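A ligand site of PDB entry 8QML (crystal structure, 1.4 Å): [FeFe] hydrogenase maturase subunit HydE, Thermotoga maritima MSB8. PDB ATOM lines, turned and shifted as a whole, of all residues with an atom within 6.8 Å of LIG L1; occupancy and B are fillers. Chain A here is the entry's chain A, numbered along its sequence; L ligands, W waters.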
ATOM      1  N   ILE A  66       5.042  -9.709   5.762  1.00  0.00           N
ATOM      2  CA  ILE A  66       6.458  -9.806   5.443  1.00  0.00           C
ATOM      3  C   ILE A  66       7.263  -9.128   6.538  1.00  0.00           C
ATOM      4  O   ILE A  66       7.036  -8.001   6.900  1.00  0.00           O
ATOM      5  CB  ILE A  66       6.743  -9.288   4.026  1.00  0.00           C
ATOM      6  CG1 ILE A  66       8.235  -9.513   3.709  1.00  0.00           C
ATOM      7  CG2 ILE A  66       6.304  -7.857   3.812  1.00  0.00           C
ATOM      8  CD1 ILE A  66       8.480  -9.328   2.200  1.00  0.00           C
ATOM      9  N   GLU A  68      11.109  -8.123   7.044  1.00  0.00           N
ATOM     10  CA  GLU A  68      12.383  -7.885   6.396  1.00  0.00           C
ATOM     11  C   GLU A  68      13.387  -7.828   7.545  1.00  0.00           C
ATOM     12  O   GLU A  68      13.561  -6.813   8.225  1.00  0.00           O
ATOM     13  CB  GLU A  68      12.227  -6.569   5.651  1.00  0.00           C
ATOM     14  CG  GLU A  68      11.219  -6.621   4.569  1.00  0.00           C
ATOM     15  CD  GLU A  68      10.663  -5.199   4.272  1.00  0.00           C
ATOM     16  OE1 GLU A  68      10.632  -4.374   5.178  1.00  0.00           O
ATOM     17  OE2 GLU A  68      10.247  -4.953   3.146  1.00  0.00           O
ATOM     18  N   VAL A 115       6.147 -14.182   5.786  1.00  0.00           N
ATOM     19  CA  VAL A 115       7.245 -14.147   4.808  1.00  0.00           C
ATOM     20  C   VAL A 115       8.449 -13.586   5.532  1.00  0.00           C
ATOM     21  O   VAL A 115       8.341 -12.516   6.121  1.00  0.00           O
ATOM     22  CB  VAL A 115       6.917 -13.225   3.648  1.00  0.00           C
ATOM     23  CG1 VAL A 115       8.050 -13.271   2.608  1.00  0.00           C
ATOM     24  CG2 VAL A 115       5.553 -13.672   2.997  1.00  0.00           C
ATOM     25  N   GLN A 117      11.968 -12.114   4.748  1.00  0.00           N
ATOM     26  CA  GLN A 117      12.788 -11.682   3.622  1.00  0.00           C
ATOM     27  C   GLN A 117      14.006 -10.953   4.151  1.00  0.00           C
ATOM     28  O   GLN A 117      13.952 -10.289   5.186  1.00  0.00           O
ATOM     29  CB  GLN A 117      12.019 -10.747   2.710  1.00  0.00           C
ATOM     30  CG  GLN A 117      12.754 -10.445   1.388  1.00  0.00           C
ATOM     31  CD  GLN A 117      11.977  -9.559   0.476  1.00  0.00           C
ATOM     32  OE1 GLN A 117      11.877  -8.358   0.732  1.00  0.00           O
ATOM     33  NE2 GLN A 117      11.393 -10.145  -0.582  1.00  0.00           N
ATOM     34  N   SER A 146      12.356 -15.652   1.646  1.00  0.00           N
ATOM     35  CA  SER A 146      12.809 -14.922   0.480  1.00  0.00           C
ATOM     36  C   SER A 146      14.175 -14.409   0.869  1.00  0.00           C
ATOM     37  O   SER A 146      14.341 -13.248   1.227  1.00  0.00           O
ATOM     38  CB  SER A 146      11.817 -13.783   0.213  1.00  0.00           C
ATOM     39  OG  SER A 146      12.171 -13.020  -0.874  1.00  0.00           O
ATOM     40  N   LEU A 167      10.327 -17.391  -2.243  1.00  0.00           N
ATOM     41  CA  LEU A 167      10.223 -16.402  -3.290  1.00  0.00           C
ATOM     42  C   LEU A 167      11.615 -16.118  -3.792  1.00  0.00           C
ATOM     43  O   LEU A 167      12.497 -15.735  -3.009  1.00  0.00           O
ATOM     44  CB  LEU A 167       9.662 -15.107  -2.743  1.00  0.00           C
ATOM     45  CG  LEU A 167       8.370 -15.225  -1.953  1.00  0.00           C
ATOM     46  CD1 LEU A 167       8.007 -13.827  -1.479  1.00  0.00           C
ATOM     47  CD2 LEU A 167       7.257 -15.786  -2.874  1.00  0.00           C
ATOM     48  N   ARG A 169      12.484 -14.156  -7.119  1.00  0.00           N
ATOM     49  CA  ARG A 169      12.130 -13.581  -8.417  1.00  0.00           C
ATOM     50  C   ARG A 169      13.245 -13.810  -9.387  1.00  0.00           C
ATOM     51  O   ARG A 169      14.409 -13.648  -9.040  1.00  0.00           O
ATOM     52  CB  ARG A 169      11.964 -12.105  -8.312  1.00  0.00           C
ATOM     53  CG  ARG A 169      10.713 -11.733  -7.540  1.00  0.00           C
ATOM     54  CD  ARG A 169      10.738 -10.231  -7.693  1.00  0.00           C
ATOM     55  NE  ARG A 169       9.610  -9.681  -6.989  1.00  0.00           N
ATOM     56  CZ  ARG A 169       9.194  -8.449  -7.204  1.00  0.00           C
ATOM     57  NH1 ARG A 169       9.964  -7.573  -7.877  1.00  0.00           N
ATOM     58  NH2 ARG A 169       8.021  -8.078  -6.727  1.00  0.00           N
ATOM     59  N   ALA A 206       8.505 -16.858  -8.545  1.00  0.00           N
ATOM     60  CA  ALA A 206       9.466 -16.150  -9.370  1.00  0.00           C
ATOM     61  C   ALA A 206       8.883 -14.783  -9.670  1.00  0.00           C
ATOM     62  O   ALA A 206       8.166 -14.210  -8.837  1.00  0.00           O
ATOM     63  CB  ALA A 206       9.713 -16.922 -10.648  1.00  0.00           C
ATOM     64  N   VAL A 235       4.037 -15.411  -8.543  1.00  0.00           N
ATOM     65  CA  VAL A 235       4.757 -14.531  -9.450  1.00  0.00           C
ATOM     66  C   VAL A 235       4.701 -13.126  -8.886  1.00  0.00           C
ATOM     67  O   VAL A 235       3.643 -12.498  -8.869  1.00  0.00           O
ATOM     68  CB  VAL A 235       4.187 -14.549 -10.877  1.00  0.00           C
ATOM     69  CG1 VAL A 235       5.036 -13.645 -11.777  1.00  0.00           C
ATOM     70  CG2 VAL A 235       4.213 -15.978 -11.415  1.00  0.00           C
ATOM     71  N   GLY A 236       5.830 -12.619  -8.408  1.00  0.00           N
ATOM     72  CA  GLY A 236       5.927 -11.273  -7.901  1.00  0.00           C
ATOM     73  C   GLY A 236       6.473 -10.368  -8.977  1.00  0.00           C
ATOM     74  O   GLY A 236       7.604 -10.562  -9.483  1.00  0.00           O
ATOM     75  N   ILE A 237       5.699  -9.353  -9.327  1.00  0.00           N
ATOM     76  CA  ILE A 237       6.063  -8.439 -10.399  1.00  0.00           C
ATOM     77  C   ILE A 237       5.910  -7.017  -9.901  1.00  0.00           C
ATOM     78  O   ILE A 237       4.936  -6.659  -9.241  1.00  0.00           O
ATOM     79  CB  ILE A 237       5.158  -8.640 -11.637  1.00  0.00           C
ATOM     80  CG1 ILE A 237       5.469  -9.985 -12.243  1.00  0.00           C
ATOM     81  CG2 ILE A 237       5.320  -7.477 -12.618  1.00  0.00           C
ATOM     82  CD1 ILE A 237       4.468 -10.357 -13.348  1.00  0.00           C
ATOM     83  N   GLY A 238       6.882  -6.195 -10.188  1.00  0.00           N
ATOM     84  CA  GLY A 238       6.716  -4.789  -9.925  1.00  0.00           C
ATOM     85  C   GLY A 238       7.647  -3.981 -10.790  1.00  0.00           C
ATOM     86  O   GLY A 238       8.473  -4.546 -11.542  1.00  0.00           O
ATOM     87  N   PRO A 239       7.460  -2.675 -10.824  1.00  0.00           N
ATOM     88  CA  PRO A 239       8.327  -1.828 -11.627  1.00  0.00           C
ATOM     89  C   PRO A 239       9.696  -1.807 -11.000  1.00  0.00           C
ATOM     90  O   PRO A 239       9.847  -2.026  -9.802  1.00  0.00           O
ATOM     91  CB  PRO A 239       7.692  -0.434 -11.482  1.00  0.00           C
ATOM     92  CG  PRO A 239       7.061  -0.513 -10.033  1.00  0.00           C
ATOM     93  CD  PRO A 239       6.487  -1.932  -9.995  1.00  0.00           C
ATOM     94  N   PRO A 276       0.923 -11.415  -6.203  1.00  0.00           N
ATOM     95  CA  PRO A 276       0.736 -10.282  -5.295  1.00  0.00           C
ATOM     96  C   PRO A 276       0.546  -8.989  -6.051  1.00  0.00           C
ATOM     97  O   PRO A 276       1.033  -8.806  -7.177  1.00  0.00           O
ATOM     98  CB  PRO A 276       2.072 -10.198  -4.535  1.00  0.00           C
ATOM     99  CG  PRO A 276       3.060 -10.774  -5.560  1.00  0.00           C
ATOM    100  CD  PRO A 276       2.300 -11.943  -6.154  1.00  0.00           C
ATOM    101  N   ALA A 277      -0.140  -8.062  -5.379  1.00  0.00           N
ATOM    102  CA  ALA A 277      -0.158  -6.673  -5.747  1.00  0.00           C
ATOM    103  C   ALA A 277       0.953  -6.075  -4.920  1.00  0.00           C
ATOM    104  O   ALA A 277       0.790  -5.877  -3.713  1.00  0.00           O
ATOM    105  CB  ALA A 277      -1.501  -6.071  -5.313  1.00  0.00           C
ATOM    106  N   THR A 278       2.121  -5.882  -5.555  1.00  0.00           N
ATOM    107  CA  THR A 278       3.303  -5.632  -4.774  1.00  0.00           C
ATOM    108  C   THR A 278       3.354  -4.216  -4.238  1.00  0.00           C
ATOM    109  O   THR A 278       2.779  -3.272  -4.755  1.00  0.00           O
ATOM    110  CB  THR A 278       4.502  -5.887  -5.652  1.00  0.00           C
ATOM    111  OG1 THR A 278       4.506  -5.028  -6.806  1.00  0.00           O
ATOM    112  CG2 THR A 278       4.568  -7.355  -6.071  1.00  0.00           C
ATOM    113  N   THR A 279       4.152  -4.062  -3.190  1.00  0.00           N
ATOM    114  CA  THR A 279       4.388  -2.748  -2.654  1.00  0.00           C
ATOM    115  C   THR A 279       4.993  -1.819  -3.686  1.00  0.00           C
ATOM    116  O   THR A 279       4.702  -0.636  -3.664  1.00  0.00           O
ATOM    117  CB  THR A 279       5.279  -2.849  -1.408  1.00  0.00           C
ATOM    118  OG1 THR A 279       4.491  -3.445  -0.383  1.00  0.00           O
ATOM    119  CG2 THR A 279       5.738  -1.448  -0.939  1.00  0.00           C
ATOM    120  N   ALA A 280       5.853  -2.332  -4.575  1.00  0.00           N
ATOM    121  CA  ALA A 280       6.426  -1.432  -5.567  1.00  0.00           C
ATOM    122  C   ALA A 280       5.329  -0.844  -6.425  1.00  0.00           C
ATOM    123  O   ALA A 280       5.389   0.334  -6.792  1.00  0.00           O
ATOM    124  CB  ALA A 280       7.429  -2.168  -6.450  1.00  0.00           C
ATOM    125  N   MET A 281       4.293  -1.644  -6.709  1.00  0.00           N
ATOM    126  CA  MET A 281       3.164  -1.092  -7.462  1.00  0.00           C
ATOM    127  C   MET A 281       2.453   0.009  -6.692  1.00  0.00           C
ATOM    128  O   MET A 281       2.092   1.029  -7.273  1.00  0.00           O
ATOM    129  CB  MET A 281       2.174  -2.214  -7.863  1.00  0.00           C
ATOM    130  CG  MET A 281       2.754  -3.074  -9.001  1.00  0.00           C
ATOM    131  SD  MET A 281       2.888  -2.237 -10.516  1.00  0.00           S
ATOM    132  CE  MET A 281       1.395  -2.730 -11.366  1.00  0.00           C
ATOM    133  N   THR A 283       3.925   1.918  -4.663  1.00  0.00           N
ATOM    134  CA  THR A 283       4.875   2.976  -4.456  1.00  0.00           C
ATOM    135  C   THR A 283       4.907   3.913  -5.643  1.00  0.00           C
ATOM    136  O   THR A 283       4.926   5.127  -5.472  1.00  0.00           O
ATOM    137  CB  THR A 283       6.231   2.340  -4.211  1.00  0.00           C
ATOM    138  OG1 THR A 283       6.143   1.615  -3.029  1.00  0.00           O
ATOM    139  CG2 THR A 283       7.252   3.465  -4.028  1.00  0.00           C
ATOM    140  N   MET A 301       0.949  -8.249   0.528  1.00  0.00           N
ATOM    141  CA  MET A 301       2.054  -8.524   1.454  1.00  0.00           C
ATOM    142  C   MET A 301       2.267  -7.308   2.359  1.00  0.00           C
ATOM    143  O   MET A 301       3.215  -6.540   2.165  1.00  0.00           O
ATOM    144  CB  MET A 301       3.275  -8.998   0.656  1.00  0.00           C
ATOM    145  CG  MET A 301       2.857 -10.092  -0.386  1.00  0.00           C
ATOM    146  SD  MET A 301       4.180 -10.563  -1.496  1.00  0.00           S
ATOM    147  CE  MET A 301       5.172 -11.527  -0.336  1.00  0.00           C
ATOM    148  N   LEU A 315      14.892  -1.301  -0.472  1.00  0.00           N
ATOM    149  CA  LEU A 315      15.305  -1.815  -1.776  1.00  0.00           C
ATOM    150  C   LEU A 315      15.218  -0.730  -2.823  1.00  0.00           C
ATOM    151  O   LEU A 315      16.067  -0.612  -3.718  1.00  0.00           O
ATOM    152  CB  LEU A 315      14.326  -2.922  -2.193  1.00  0.00           C
ATOM    153  CG  LEU A 315      14.156  -4.031  -1.197  1.00  0.00           C
ATOM    154  CD1 LEU A 315      13.020  -4.893  -1.696  1.00  0.00           C
ATOM    155  CD2 LEU A 315      15.487  -4.821  -1.258  1.00  0.00           C
ATOM    156  N   TYR A 316      14.174   0.078  -2.746  1.00  0.00           N
ATOM    157  CA  TYR A 316      14.030   1.252  -3.575  1.00  0.00           C
ATOM    158  C   TYR A 316      13.421   2.315  -2.678  1.00  0.00           C
ATOM    159  O   TYR A 316      12.875   1.998  -1.605  1.00  0.00           O
ATOM    160  CB  TYR A 316      13.080   0.938  -4.755  1.00  0.00           C
ATOM    161  CG  TYR A 316      11.807   0.282  -4.293  1.00  0.00           C
ATOM    162  CD1 TYR A 316      10.748   1.043  -3.802  1.00  0.00           C
ATOM    163  CD2 TYR A 316      11.659  -1.109  -4.315  1.00  0.00           C
ATOM    164  CE1 TYR A 316       9.597   0.441  -3.340  1.00  0.00           C
ATOM    165  CE2 TYR A 316      10.544  -1.721  -3.860  1.00  0.00           C
ATOM    166  CZ  TYR A 316       9.467  -0.936  -3.363  1.00  0.00           C
ATOM    167  OH  TYR A 316       8.320  -1.538  -2.924  1.00  0.00           O
HETATM  168  O1  LIG L   1       7.129 -10.922  -3.314  1.00  0.00           O
HETATM  169  C1  LIG L   1       7.151  -9.734  -3.713  1.00  0.00           C
HETATM  170  O2  LIG L   1       6.589  -9.372  -4.786  1.00  0.00           O
HETATM  171  C2  LIG L   1       7.884  -8.750  -2.835  1.00  0.00           C
HETATM  172  C3  LIG L   1       7.746  -9.127  -1.338  1.00  0.00           C
HETATM  173  N1  LIG L   1       7.323  -7.427  -3.079  1.00  0.00           N
HETATM  174  S1  LIG L   1       9.606  -8.633  -3.286  1.00  0.00           S
HETATM  175  C4  LIG L   1       9.675  -6.886  -3.512  1.00  0.00           C
HETATM  176  C5  LIG L   1       8.380  -6.428  -2.802  1.00  0.00           C
HETATM  177  C6  LIG L   1       8.018  -5.027  -3.200  1.00  0.00           C
HETATM  178  O3  LIG L   1       7.235  -4.844  -4.143  1.00  0.00           O
HETATM  179  O4  LIG L   1       8.517  -4.063  -2.607  1.00  0.00           O
HETATM  180  N1  LG2 L   2      17.828 -10.746  -1.354  1.00  0.00           N
HETATM  181  C1  LG2 L   2      16.608 -11.429  -1.826  1.00  0.00           C
HETATM  182  C2  LG2 L   2      15.326 -10.853  -1.237  1.00  0.00           C
HETATM  183  C3  LG2 L   2      15.194  -9.321  -1.163  1.00  0.00           C
HETATM  184  S1  LG2 L   2      15.169  -8.433  -2.748  1.00  0.00           S
HETATM  185  C4  LG2 L   2      16.601 -11.533  -3.322  1.00  0.00           C
HETATM  186  O1  LG2 L   2      17.356 -10.840  -4.042  1.00  0.00           O
HETATM  187  O2  LG2 L   2      15.843 -12.379  -3.831  1.00  0.00           O
HETATM  188  C5  LG2 L   2      13.430  -8.701  -3.186  1.00  0.00           C
HETATM  189  C6  LG2 L   2      13.052  -8.164  -4.579  1.00  0.00           C
HETATM  190  O3  LG2 L   2      13.087  -6.750  -4.549  1.00  0.00           O
HETATM  191  C7  LG2 L   2      14.062  -8.503  -5.667  1.00  0.00           C
HETATM  192  O4  LG2 L   2      13.744  -9.809  -6.129  1.00  0.00           O
HETATM  193  C8  LG2 L   2      13.828  -7.402  -6.690  1.00  0.00           C
HETATM  194  O5  LG2 L   2      12.999  -7.799  -7.782  1.00  0.00           O
HETATM  195  C9  LG2 L   2      13.128  -6.294  -5.872  1.00  0.00           C
HETATM  196  N2  LG2 L   2      13.873  -5.045  -5.961  1.00  0.00           N
HETATM  197  C10 LG2 L   2      15.217  -4.835  -5.579  1.00  0.00           C
HETATM  198  N3  LG2 L   2      15.567  -3.602  -5.889  1.00  0.00           N
HETATM  199  C11 LG2 L   2      14.497  -2.998  -6.531  1.00  0.00           C
HETATM  200  C12 LG2 L   2      14.307  -1.717  -7.054  1.00  0.00           C
HETATM  201  N4  LG2 L   2      15.266  -0.768  -7.069  1.00  0.00           N
HETATM  202  N5  LG2 L   2      13.104  -1.404  -7.640  1.00  0.00           N
HETATM  203  C13 LG2 L   2      12.087  -2.335  -7.678  1.00  0.00           C
HETATM  204  N6  LG2 L   2      12.236  -3.597  -7.133  1.00  0.00           N
HETATM  205  C14 LG2 L   2      13.448  -3.923  -6.572  1.00  0.00           C
HETATM  206  O   HOH W   1       8.876 -11.924  -4.940  1.00  0.00           O
HETATM  207  O   HOH W   2       7.649  -5.458  -6.764  1.00  0.00           O
HETATM  208  O   HOH W   3       9.929  -3.940  -0.399  1.00  0.00           O
HETATM  209  O   HOH W   4       5.686 -12.992  -4.779  1.00  0.00           O
HETATM  210  O   HOH W   5       4.947  -6.487  -1.922  1.00  0.00           O
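The side-chain hydroxyl of Tyr 316 lies within hydrogen-bond range of an oxygen (O4) of LIG L1, 2.6 Å away.
The guanidinium group (NH2) of Arg 169 lies within salt-bridge range of an oxygen (O2) of LIG L1 (2.7 Å).
O3 of LIG L1 sits at hydrogen-bond distance from N of Ala 280 (2.9 Å).
The backbone NH (N) of Thr 279 sits at hydrogen-bond distance from an oxygen (O3) of LIG L1 (3.3 Å).
NE2 of Gln 117 lies close to S1 of LIG L1 (3.6 Å).
NH1 of Arg 169 lies within hydrogen-bond range of O5 of LG2 L2 (3.0 Å).
The backbone carbonyl oxygen of Leu 315 is in hydrogen-bond range of a nitrogen (N4) of LG2 L2 (3.4 Å).
The side-chain hydroxyl of Tyr 316 is in hydrogen-bond range of the backbone NH of Ala 280, at 3.1 Å.
The guanidinium group (NE) of Arg 169 lies within hydrogen-bond range of the backbone carbonyl oxygen (O) of Gly 236.
The side-chain hydroxyl (OG1) of Thr 278 lies within hydrogen-bond range of the backbone carbonyl oxygen (O) of Ile 237 (3.0 Å).
OG1 of Thr 278 sits at hydrogen-bond distance from N of Met 281.
OG1 of Thr 283 sits at hydrogen-bond distance from O of Thr 279 (2.7 Å).
The backbone carbonyl oxygen (O) of Leu 167 is in hydrogen-bond range of the side-chain hydroxyl (OG) of Ser 146 (3.5 Å).
The side-chain hydroxyl of Ser 146 sits at hydrogen-bond distance from the side-chain amide nitrogen of Gln 117 (3.0 Å).
The backbone carbonyl oxygen (O) of Ala 206 is in hydrogen-bond range of the backbone NH (N) of Gly 236 (2.9 Å).
O1 of LIG L1 sits close to SD of Met 301, 3.5 Å away.
Merely in contact with LIG L1: Thr 278, Leu 167, Ile 66, Gly 236 and Pro 276.
Hydrophobic or aromatic side chains that line LIG L1: Ile 66, Leu 167, Pro 276, Ala 280, Met 301 and Tyr 316.
Within 4 Å of LIG L1: Ile 66, Gln 117, Leu 167, Arg 169, Gly 236, Pro 276, Thr 278, Thr 279, Ala 280, Met 301 and Tyr 316.
Water W1 bridges O1 of LIG L1 and NE of Arg 169.
Water W2 lies within hydrogen-bond range of the guanidinium group of Arg 169 (2.6 Å), an oxygen (O3) of LIG L1 (2.7 Å) and the side-chain hydroxyl of Thr 278 (3.2 Å).
Water W5 bridges a nitrogen (N1) of LIG L1 (2.8 Å) and the backbone NH (N) of Thr 279 (2.8 Å).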
